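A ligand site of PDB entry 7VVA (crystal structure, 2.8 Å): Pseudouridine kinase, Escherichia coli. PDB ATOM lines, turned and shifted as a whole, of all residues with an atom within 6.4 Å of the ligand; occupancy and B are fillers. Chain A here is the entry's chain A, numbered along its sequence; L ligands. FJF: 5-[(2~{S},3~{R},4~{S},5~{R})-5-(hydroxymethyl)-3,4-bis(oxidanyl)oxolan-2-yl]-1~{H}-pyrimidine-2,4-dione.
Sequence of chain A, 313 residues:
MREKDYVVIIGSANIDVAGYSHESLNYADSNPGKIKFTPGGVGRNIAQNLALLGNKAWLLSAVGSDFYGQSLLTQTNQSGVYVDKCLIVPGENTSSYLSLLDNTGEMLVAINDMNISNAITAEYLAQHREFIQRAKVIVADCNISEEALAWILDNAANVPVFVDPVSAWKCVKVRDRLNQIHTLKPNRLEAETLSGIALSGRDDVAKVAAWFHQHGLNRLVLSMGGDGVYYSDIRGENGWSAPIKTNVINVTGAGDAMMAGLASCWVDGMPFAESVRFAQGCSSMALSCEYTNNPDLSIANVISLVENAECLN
SD of Met 114 lies within hydrogen-bond range of ND2 of Asn 14, 3.1 Å away.
O of Gly 41 lies close to OD1 of Asn 45 (3.3 Å).
The side-chain amino group (NZ) of Lys 170 sits close to the side-chain amide nitrogen (ND2) of Asn 112.
N of Tyr 97 sits at hydrogen-bond distance from O of Ile 15 (2.9 Å).
OD2 of Asp 256 sits at hydrogen-bond distance from ND2 of Asn 45 (3.2 Å).
ND2 of Asn 143 lies within hydrogen-bond range of OD2 of Asp 141 (3.2 Å).
NZ of Lys 170 sits at hydrogen-bond distance from OD1 of Asn 143 (2.9 Å).
N of Gly 40 lies within hydrogen-bond range of O of Asn 14, 2.9 Å away.
Merely in contact with the ligand: Val 166 (3.4 Å), Tyr 97 (3.5 Å), Thr 252 (3.5 Å), Asn 112 (3.7 Å), Gly 253 (3.7 Å), Asn 14 (3.7 Å), Gly 40 (3.8 Å), Ser 167 (3.8 Å) and Asn 45 (3.9 Å).
Hydrophobic or aromatic side chains within 4 Å of the ligand: Val 42, Tyr 97, Met 114 and Val 166.
16 residues have an atom within 4 Å of the ligand: Asn 14, Asp 16, Gly 40, Gly 41, Val 42, Asn 45, Tyr 97, Asn 112, Met 114, Asn 143, Val 166, Ser 167, Lys 170, Thr 252, Gly 253 and Asp 256.
OD2 of Asp 256 is in hydrogen-bond range of O13 of the ligand, 3.0 Å away.
OD2 of Asp 16 lies within hydrogen-bond range of O17 of the ligand.
The side-chain sulfur (SD) of Met 114 sits at hydrogen-bond distance from a nitrogen (N08) of the ligand (3.5 Å).
The side-chain amide nitrogen (ND2) of Asn 143 sits at hydrogen-bond distance from an oxygen (O07) of the ligand, 2.8 Å away.
An oxygen (O01) of the ligand is in hydrogen-bond range of the side-chain amino group of Lys 170 (3.4 Å).
N of Gly 41 is in hydrogen-bond range of O17 of the ligand (2.9 Å).
N of Val 42 sits close to O10 of the ligand, 3.3 Å away.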
ATOM      1  N   SER A  12     -13.030   0.301  32.066  1.00  0.00           N
ATOM      2  CA  SER A  12     -14.381   0.540  31.570  1.00  0.00           C
ATOM      3  C   SER A  12     -14.656  -0.207  30.262  1.00  0.00           C
ATOM      4  O   SER A  12     -13.750  -0.485  29.479  1.00  0.00           O
ATOM      5  CB  SER A  12     -14.619   2.033  31.376  1.00  0.00           C
ATOM      6  OG  SER A  12     -14.675   2.699  32.620  1.00  0.00           O
ATOM      7  N   ASN A  14     -17.139   0.286  27.046  1.00  0.00           N
ATOM      8  CA  ASN A  14     -18.069   1.190  26.390  1.00  0.00           C
ATOM      9  C   ASN A  14     -18.596   0.673  25.049  1.00  0.00           C
ATOM     10  O   ASN A  14     -17.969  -0.175  24.418  1.00  0.00           O
ATOM     11  CB  ASN A  14     -17.406   2.557  26.173  1.00  0.00           C
ATOM     12  CG  ASN A  14     -16.848   3.145  27.459  1.00  0.00           C
ATOM     13  OD1 ASN A  14     -17.033   2.592  28.541  1.00  0.00           O
ATOM     14  ND2 ASN A  14     -16.167   4.278  27.331  1.00  0.00           N
ATOM     15  N   ILE A  15     -19.745   1.192  24.628  1.00  0.00           N
ATOM     16  CA  ILE A  15     -20.213   0.978  23.262  1.00  0.00           C
ATOM     17  C   ILE A  15     -19.788   2.164  22.401  1.00  0.00           C
ATOM     18  O   ILE A  15     -20.220   3.303  22.623  1.00  0.00           O
ATOM     19  CB  ILE A  15     -21.746   0.752  23.181  1.00  0.00           C
ATOM     20  CG1 ILE A  15     -22.214   0.841  21.728  1.00  0.00           C
ATOM     21  CG2 ILE A  15     -22.503   1.720  24.063  1.00  0.00           C
ATOM     22  CD1 ILE A  15     -21.783  -0.331  20.873  1.00  0.00           C
ATOM     23  N   ASP A  16     -18.922   1.897  21.438  1.00  0.00           N
ATOM     24  CA  ASP A  16     -18.335   2.935  20.589  1.00  0.00           C
ATOM     25  C   ASP A  16     -19.134   3.168  19.315  1.00  0.00           C
ATOM     26  O   ASP A  16     -19.350   2.251  18.531  1.00  0.00           O
ATOM     27  CB  ASP A  16     -16.903   2.571  20.228  1.00  0.00           C
ATOM     28  CG  ASP A  16     -15.965   2.645  21.414  1.00  0.00           C
ATOM     29  OD1 ASP A  16     -16.446   2.587  22.565  1.00  0.00           O
ATOM     30  OD2 ASP A  16     -14.737   2.741  21.193  1.00  0.00           O
ATOM     31  N   PRO A  39     -17.197  -2.586  19.912  1.00  0.00           N
ATOM     32  CA  PRO A  39     -16.800  -2.677  21.329  1.00  0.00           C
ATOM     33  C   PRO A  39     -15.666  -1.721  21.682  1.00  0.00           C
ATOM     34  O   PRO A  39     -14.741  -1.542  20.875  1.00  0.00           O
ATOM     35  CB  PRO A  39     -16.359  -4.139  21.481  1.00  0.00           C
ATOM     36  CG  PRO A  39     -16.039  -4.586  20.089  1.00  0.00           C
ATOM     37  CD  PRO A  39     -17.027  -3.869  19.215  1.00  0.00           C
ATOM     38  N   GLY A  40     -15.726  -1.109  22.855  1.00  0.00           N
ATOM     39  CA  GLY A  40     -14.738  -0.139  23.259  1.00  0.00           C
ATOM     40  C   GLY A  40     -14.528  -0.061  24.756  1.00  0.00           C
ATOM     41  O   GLY A  40     -14.980  -0.927  25.503  1.00  0.00           O
ATOM     42  N   GLY A  41     -13.836   0.991  25.200  1.00  0.00           N
ATOM     43  CA  GLY A  41     -13.483   1.146  26.598  1.00  0.00           C
ATOM     44  C   GLY A  41     -12.035   0.761  26.814  1.00  0.00           C
ATOM     45  O   GLY A  41     -11.615  -0.332  26.450  1.00  0.00           O
ATOM     46  N   VAL A  42     -11.265   1.679  27.397  1.00  0.00           N
ATOM     47  CA  VAL A  42      -9.836   1.500  27.612  1.00  0.00           C
ATOM     48  C   VAL A  42      -9.484   0.148  28.255  1.00  0.00           C
ATOM     49  O   VAL A  42      -8.733  -0.642  27.679  1.00  0.00           O
ATOM     50  CB  VAL A  42      -9.257   2.632  28.485  1.00  0.00           C
ATOM     51  CG1 VAL A  42      -7.822   2.332  28.879  1.00  0.00           C
ATOM     52  CG2 VAL A  42      -9.339   3.948  27.747  1.00  0.00           C
ATOM     53  N   GLY A  43     -10.049  -0.105  29.429  1.00  0.00           N
ATOM     54  CA  GLY A  43      -9.796  -1.330  30.157  1.00  0.00           C
ATOM     55  C   GLY A  43     -10.158  -2.578  29.378  1.00  0.00           C
ATOM     56  O   GLY A  43      -9.392  -3.549  29.340  1.00  0.00           O
ATOM     57  N   ASN A  45     -10.423  -2.916  26.111  1.00  0.00           N
ATOM     58  CA  ASN A  45      -9.515  -3.066  24.981  1.00  0.00           C
ATOM     59  C   ASN A  45      -8.172  -3.632  25.422  1.00  0.00           C
ATOM     60  O   ASN A  45      -7.630  -4.545  24.790  1.00  0.00           O
ATOM     61  CB  ASN A  45      -9.304  -1.730  24.268  1.00  0.00           C
ATOM     62  CG  ASN A  45     -10.595  -1.165  23.696  1.00  0.00           C
ATOM     63  OD1 ASN A  45     -11.597  -1.872  23.573  1.00  0.00           O
ATOM     64  ND2 ASN A  45     -10.570   0.103  23.322  1.00  0.00           N
ATOM     65  N   TYR A  97     -19.403   5.821  23.858  1.00  0.00           N
ATOM     66  CA  TYR A  97     -18.378   6.745  23.353  1.00  0.00           C
ATOM     67  C   TYR A  97     -18.641   7.109  21.898  1.00  0.00           C
ATOM     68  O   TYR A  97     -18.508   6.278  21.007  1.00  0.00           O
ATOM     69  CB  TYR A  97     -17.000   6.104  23.512  1.00  0.00           C
ATOM     70  CG  TYR A  97     -15.839   6.911  22.948  1.00  0.00           C
ATOM     71  CD1 TYR A  97     -15.437   8.099  23.534  1.00  0.00           C
ATOM     72  CD2 TYR A  97     -15.150   6.468  21.831  1.00  0.00           C
ATOM     73  CE1 TYR A  97     -14.379   8.834  23.019  1.00  0.00           C
ATOM     74  CE2 TYR A  97     -14.088   7.194  21.306  1.00  0.00           C
ATOM     75  CZ  TYR A  97     -13.709   8.368  21.906  1.00  0.00           C
ATOM     76  OH  TYR A  97     -12.656   9.090  21.391  1.00  0.00           O
ATOM     77  N   SER A  99     -17.553   9.176  18.594  1.00  0.00           N
ATOM     78  CA  SER A  99     -16.336   9.724  18.006  1.00  0.00           C
ATOM     79  C   SER A  99     -16.443   9.940  16.492  1.00  0.00           C
ATOM     80  O   SER A  99     -16.916   9.059  15.775  1.00  0.00           O
ATOM     81  CB  SER A  99     -15.162   8.812  18.347  1.00  0.00           C
ATOM     82  OG  SER A  99     -15.522   7.450  18.179  1.00  0.00           O
ATOM     83  N   ALA A 110     -14.539  14.270  20.624  1.00  0.00           N
ATOM     84  CA  ALA A 110     -15.008  12.985  21.114  1.00  0.00           C
ATOM     85  C   ALA A 110     -15.845  13.179  22.382  1.00  0.00           C
ATOM     86  O   ALA A 110     -15.440  13.887  23.290  1.00  0.00           O
ATOM     87  CB  ALA A 110     -13.849  12.054  21.375  1.00  0.00           C
ATOM     88  N   ASN A 112     -17.986  11.281  25.599  1.00  0.00           N
ATOM     89  CA  ASN A 112     -18.142  10.030  26.334  1.00  0.00           C
ATOM     90  C   ASN A 112     -19.210  10.136  27.422  1.00  0.00           C
ATOM     91  O   ASN A 112     -19.166  11.025  28.267  1.00  0.00           O
ATOM     92  CB  ASN A 112     -16.817   9.590  26.952  1.00  0.00           C
ATOM     93  CG  ASN A 112     -16.141  10.704  27.738  1.00  0.00           C
ATOM     94  OD1 ASN A 112     -15.561  11.614  27.162  1.00  0.00           O
ATOM     95  ND2 ASN A 112     -16.220  10.626  29.068  1.00  0.00           N
ATOM     96  N   MET A 114     -20.163   8.056  30.282  1.00  0.00           N
ATOM     97  CA  MET A 114     -19.732   6.953  31.136  1.00  0.00           C
ATOM     98  C   MET A 114     -20.037   7.259  32.597  1.00  0.00           C
ATOM     99  O   MET A 114     -19.246   7.913  33.280  1.00  0.00           O
ATOM    100  CB  MET A 114     -18.234   6.698  30.952  1.00  0.00           C
ATOM    101  CG  MET A 114     -17.788   6.716  29.508  1.00  0.00           C
ATOM    102  SD  MET A 114     -15.997   6.565  29.350  1.00  0.00           S
ATOM    103  CE  MET A 114     -15.674   5.262  30.525  1.00  0.00           C
ATOM    104  N   ASP A 141      -7.393   1.730  34.779  1.00  0.00           N
ATOM    105  CA  ASP A 141      -7.470   2.968  34.017  1.00  0.00           C
ATOM    106  C   ASP A 141      -8.117   4.058  34.875  1.00  0.00           C
ATOM    107  O   ASP A 141      -8.729   3.767  35.903  1.00  0.00           O
ATOM    108  CB  ASP A 141      -8.219   2.768  32.679  1.00  0.00           C
ATOM    109  CG  ASP A 141      -9.691   2.426  32.857  1.00  0.00           C
ATOM    110  OD1 ASP A 141     -10.227   2.503  33.989  1.00  0.00           O
ATOM    111  OD2 ASP A 141     -10.330   2.084  31.843  1.00  0.00           O
ATOM    112  N   ASN A 143     -10.699   5.791  34.404  1.00  0.00           N
ATOM    113  CA  ASN A 143     -12.127   5.977  34.153  1.00  0.00           C
ATOM    114  C   ASN A 143     -12.960   5.650  35.393  1.00  0.00           C
ATOM    115  O   ASN A 143     -14.113   6.056  35.508  1.00  0.00           O
ATOM    116  CB  ASN A 143     -12.584   5.108  32.983  1.00  0.00           C
ATOM    117  CG  ASN A 143     -12.185   5.674  31.636  1.00  0.00           C
ATOM    118  OD1 ASN A 143     -12.339   6.865  31.389  1.00  0.00           O
ATOM    119  ND2 ASN A 143     -11.663   4.817  30.769  1.00  0.00           N
ATOM    120  N   VAL A 166      -5.907   7.505  30.460  1.00  0.00           N
ATOM    121  CA  VAL A 166      -7.104   7.720  29.640  1.00  0.00           C
ATOM    122  C   VAL A 166      -7.227   9.150  29.123  1.00  0.00           C
ATOM    123  O   VAL A 166      -7.088   9.391  27.926  1.00  0.00           O
ATOM    124  CB  VAL A 166      -8.426   7.356  30.387  1.00  0.00           C
ATOM    125  CG1 VAL A 166      -9.532   7.080  29.401  1.00  0.00           C
ATOM    126  CG2 VAL A 166      -8.219   6.169  31.315  1.00  0.00           C
ATOM    127  N   SER A 167      -7.470  10.095  30.026  1.00  0.00           N
ATOM    128  CA  SER A 167      -7.625  11.496  29.637  1.00  0.00           C
ATOM    129  C   SER A 167      -6.848  12.421  30.563  1.00  0.00           C
ATOM    130  O   SER A 167      -6.444  12.028  31.660  1.00  0.00           O
ATOM    131  CB  SER A 167      -9.107  11.878  29.634  1.00  0.00           C
ATOM    132  OG  SER A 167      -9.777  11.340  28.511  1.00  0.00           O
ATOM    133  N   TRP A 169      -7.969  15.262  31.927  1.00  0.00           N
ATOM    134  CA  TRP A 169      -8.817  15.731  33.018  1.00  0.00           C
ATOM    135  C   TRP A 169      -9.145  14.592  33.994  1.00  0.00           C
ATOM    136  O   TRP A 169      -9.595  14.841  35.108  1.00  0.00           O
ATOM    137  CB  TRP A 169     -10.108  16.372  32.485  1.00  0.00           C
ATOM    138  CG  TRP A 169     -11.113  15.433  31.880  1.00  0.00           C
ATOM    139  CD1 TRP A 169     -11.114  14.935  30.605  1.00  0.00           C
ATOM    140  CD2 TRP A 169     -12.284  14.899  32.514  1.00  0.00           C
ATOM    141  NE1 TRP A 169     -12.207  14.126  30.411  1.00  0.00           N
ATOM    142  CE2 TRP A 169     -12.934  14.083  31.564  1.00  0.00           C
ATOM    143  CE3 TRP A 169     -12.848  15.029  33.788  1.00  0.00           C
ATOM    144  CZ2 TRP A 169     -14.117  13.392  31.855  1.00  0.00           C
ATOM    145  CZ3 TRP A 169     -14.016  14.348  34.076  1.00  0.00           C
ATOM    146  CH2 TRP A 169     -14.643  13.545  33.112  1.00  0.00           C
ATOM    147  N   LYS A 170      -8.940  13.355  33.552  1.00  0.00           N
ATOM    148  CA  LYS A 170      -9.233  12.199  34.395  1.00  0.00           C
ATOM    149  C   LYS A 170      -7.986  11.578  35.035  1.00  0.00           C
ATOM    150  O   LYS A 170      -8.112  10.675  35.865  1.00  0.00           O
ATOM    151  CB  LYS A 170      -9.952  11.117  33.582  1.00  0.00           C
ATOM    152  CG  LYS A 170     -11.432  11.347  33.360  1.00  0.00           C
ATOM    153  CD  LYS A 170     -11.968  10.332  32.351  1.00  0.00           C
ATOM    154  CE  LYS A 170     -13.426   9.993  32.592  1.00  0.00           C
ATOM    155  NZ  LYS A 170     -14.021   9.280  31.432  1.00  0.00           N
ATOM    156  N   VAL A 251      -6.278   5.358  14.276  1.00  0.00           N
ATOM    157  CA  VAL A 251      -5.392   5.680  15.386  1.00  0.00           C
ATOM    158  C   VAL A 251      -5.891   5.092  16.704  1.00  0.00           C
ATOM    159  O   VAL A 251      -5.185   5.117  17.722  1.00  0.00           O
ATOM    160  CB  VAL A 251      -5.218   7.214  15.538  1.00  0.00           C
ATOM    161  CG1 VAL A 251      -6.366   7.811  16.339  1.00  0.00           C
ATOM    162  CG2 VAL A 251      -3.878   7.539  16.182  1.00  0.00           C
ATOM    163  N   THR A 252      -7.110   4.567  16.688  1.00  0.00           N
ATOM    164  CA  THR A 252      -7.744   4.061  17.894  1.00  0.00           C
ATOM    165  C   THR A 252      -7.103   2.756  18.371  1.00  0.00           C
ATOM    166  O   THR A 252      -6.870   1.849  17.581  1.00  0.00           O
ATOM    167  CB  THR A 252      -9.256   3.823  17.670  1.00  0.00           C
ATOM    168  OG1 THR A 252      -9.835   4.969  17.043  1.00  0.00           O
ATOM    169  CG2 THR A 252      -9.965   3.540  18.978  1.00  0.00           C
ATOM    170  N   GLY A 253      -6.828   2.673  19.672  1.00  0.00           N
ATOM    171  CA  GLY A 253      -6.298   1.454  20.247  1.00  0.00           C
ATOM    172  C   GLY A 253      -4.790   1.403  20.472  1.00  0.00           C
ATOM    173  O   GLY A 253      -4.270   0.391  20.946  1.00  0.00           O
ATOM    174  N   ALA A 254      -4.090   2.485  20.145  1.00  0.00           N
ATOM    175  CA  ALA A 254      -2.627   2.511  20.258  1.00  0.00           C
ATOM    176  C   ALA A 254      -2.151   2.342  21.699  1.00  0.00           C
ATOM    177  O   ALA A 254      -1.376   1.422  21.993  1.00  0.00           O
ATOM    178  CB  ALA A 254      -2.086   3.810  19.670  1.00  0.00           C
ATOM    179  N   GLY A 255      -2.599   3.224  22.581  1.00  0.00           N
ATOM    180  CA  GLY A 255      -2.163   3.200  23.969  1.00  0.00           C
ATOM    181  C   GLY A 255      -2.580   1.947  24.716  1.00  0.00           C
ATOM    182  O   GLY A 255      -1.868   1.487  25.612  1.00  0.00           O
ATOM    183  N   ASP A 256      -3.718   1.380  24.323  1.00  0.00           N
ATOM    184  CA  ASP A 256      -4.210   0.153  24.933  1.00  0.00           C
ATOM    185  C   ASP A 256      -3.283  -1.014  24.594  1.00  0.00           C
ATOM    186  O   ASP A 256      -2.956  -1.839  25.445  1.00  0.00           O
ATOM    187  CB  ASP A 256      -5.637  -0.140  24.479  1.00  0.00           C
ATOM    188  CG  ASP A 256      -6.597   0.993  24.795  1.00  0.00           C
ATOM    189  OD1 ASP A 256      -6.347   1.719  25.786  1.00  0.00           O
ATOM    190  OD2 ASP A 256      -7.594   1.168  24.061  1.00  0.00           O
ATOM    191  N   THR A 292     -10.507  -1.354  16.181  1.00  0.00           N
ATOM    192  CA  THR A 292      -9.910  -0.852  17.422  1.00  0.00           C
ATOM    193  C   THR A 292      -8.884  -1.868  17.906  1.00  0.00           C
ATOM    194  O   THR A 292      -7.789  -1.504  18.344  1.00  0.00           O
ATOM    195  CB  THR A 292     -10.964  -0.598  18.507  1.00  0.00           C
ATOM    196  OG1 THR A 292     -11.575  -1.837  18.877  1.00  0.00           O
ATOM    197  CG2 THR A 292     -12.024   0.378  18.007  1.00  0.00           C
HETATM  198  O01 FJF L   1     -12.862   9.088  28.228  1.00  0.00           O
HETATM  199  C02 FJF L   1     -12.761   8.069  27.575  1.00  0.00           C
HETATM  200  N03 FJF L   1     -12.715   8.137  26.233  1.00  0.00           N
HETATM  201  C04 FJF L   1     -12.611   7.031  25.471  1.00  0.00           C
HETATM  202  C05 FJF L   1     -12.547   5.795  26.104  1.00  0.00           C
HETATM  203  C06 FJF L   1     -12.592   5.751  27.486  1.00  0.00           C
HETATM  204  O07 FJF L   1     -12.545   4.688  28.068  1.00  0.00           O
HETATM  205  N08 FJF L   1     -12.703   6.889  28.193  1.00  0.00           N
HETATM  206  C09 FJF L   1     -12.425   4.467  25.298  1.00  0.00           C
HETATM  207  O10 FJF L   1     -11.220   4.108  25.118  1.00  0.00           O
HETATM  208  C11 FJF L   1     -10.955   3.960  23.530  1.00  0.00           C
HETATM  209  C12 FJF L   1      -9.629   4.583  23.146  1.00  0.00           C
HETATM  210  O13 FJF L   1      -8.762   3.538  22.728  1.00  0.00           O
HETATM  211  C14 FJF L   1     -11.916   4.566  22.935  1.00  0.00           C
HETATM  212  O15 FJF L   1     -12.265   3.947  21.598  1.00  0.00           O
HETATM  213  C16 FJF L   1     -13.089   4.582  23.906  1.00  0.00           C
HETATM  214  O17 FJF L   1     -13.894   3.505  23.707  1.00  0.00           O
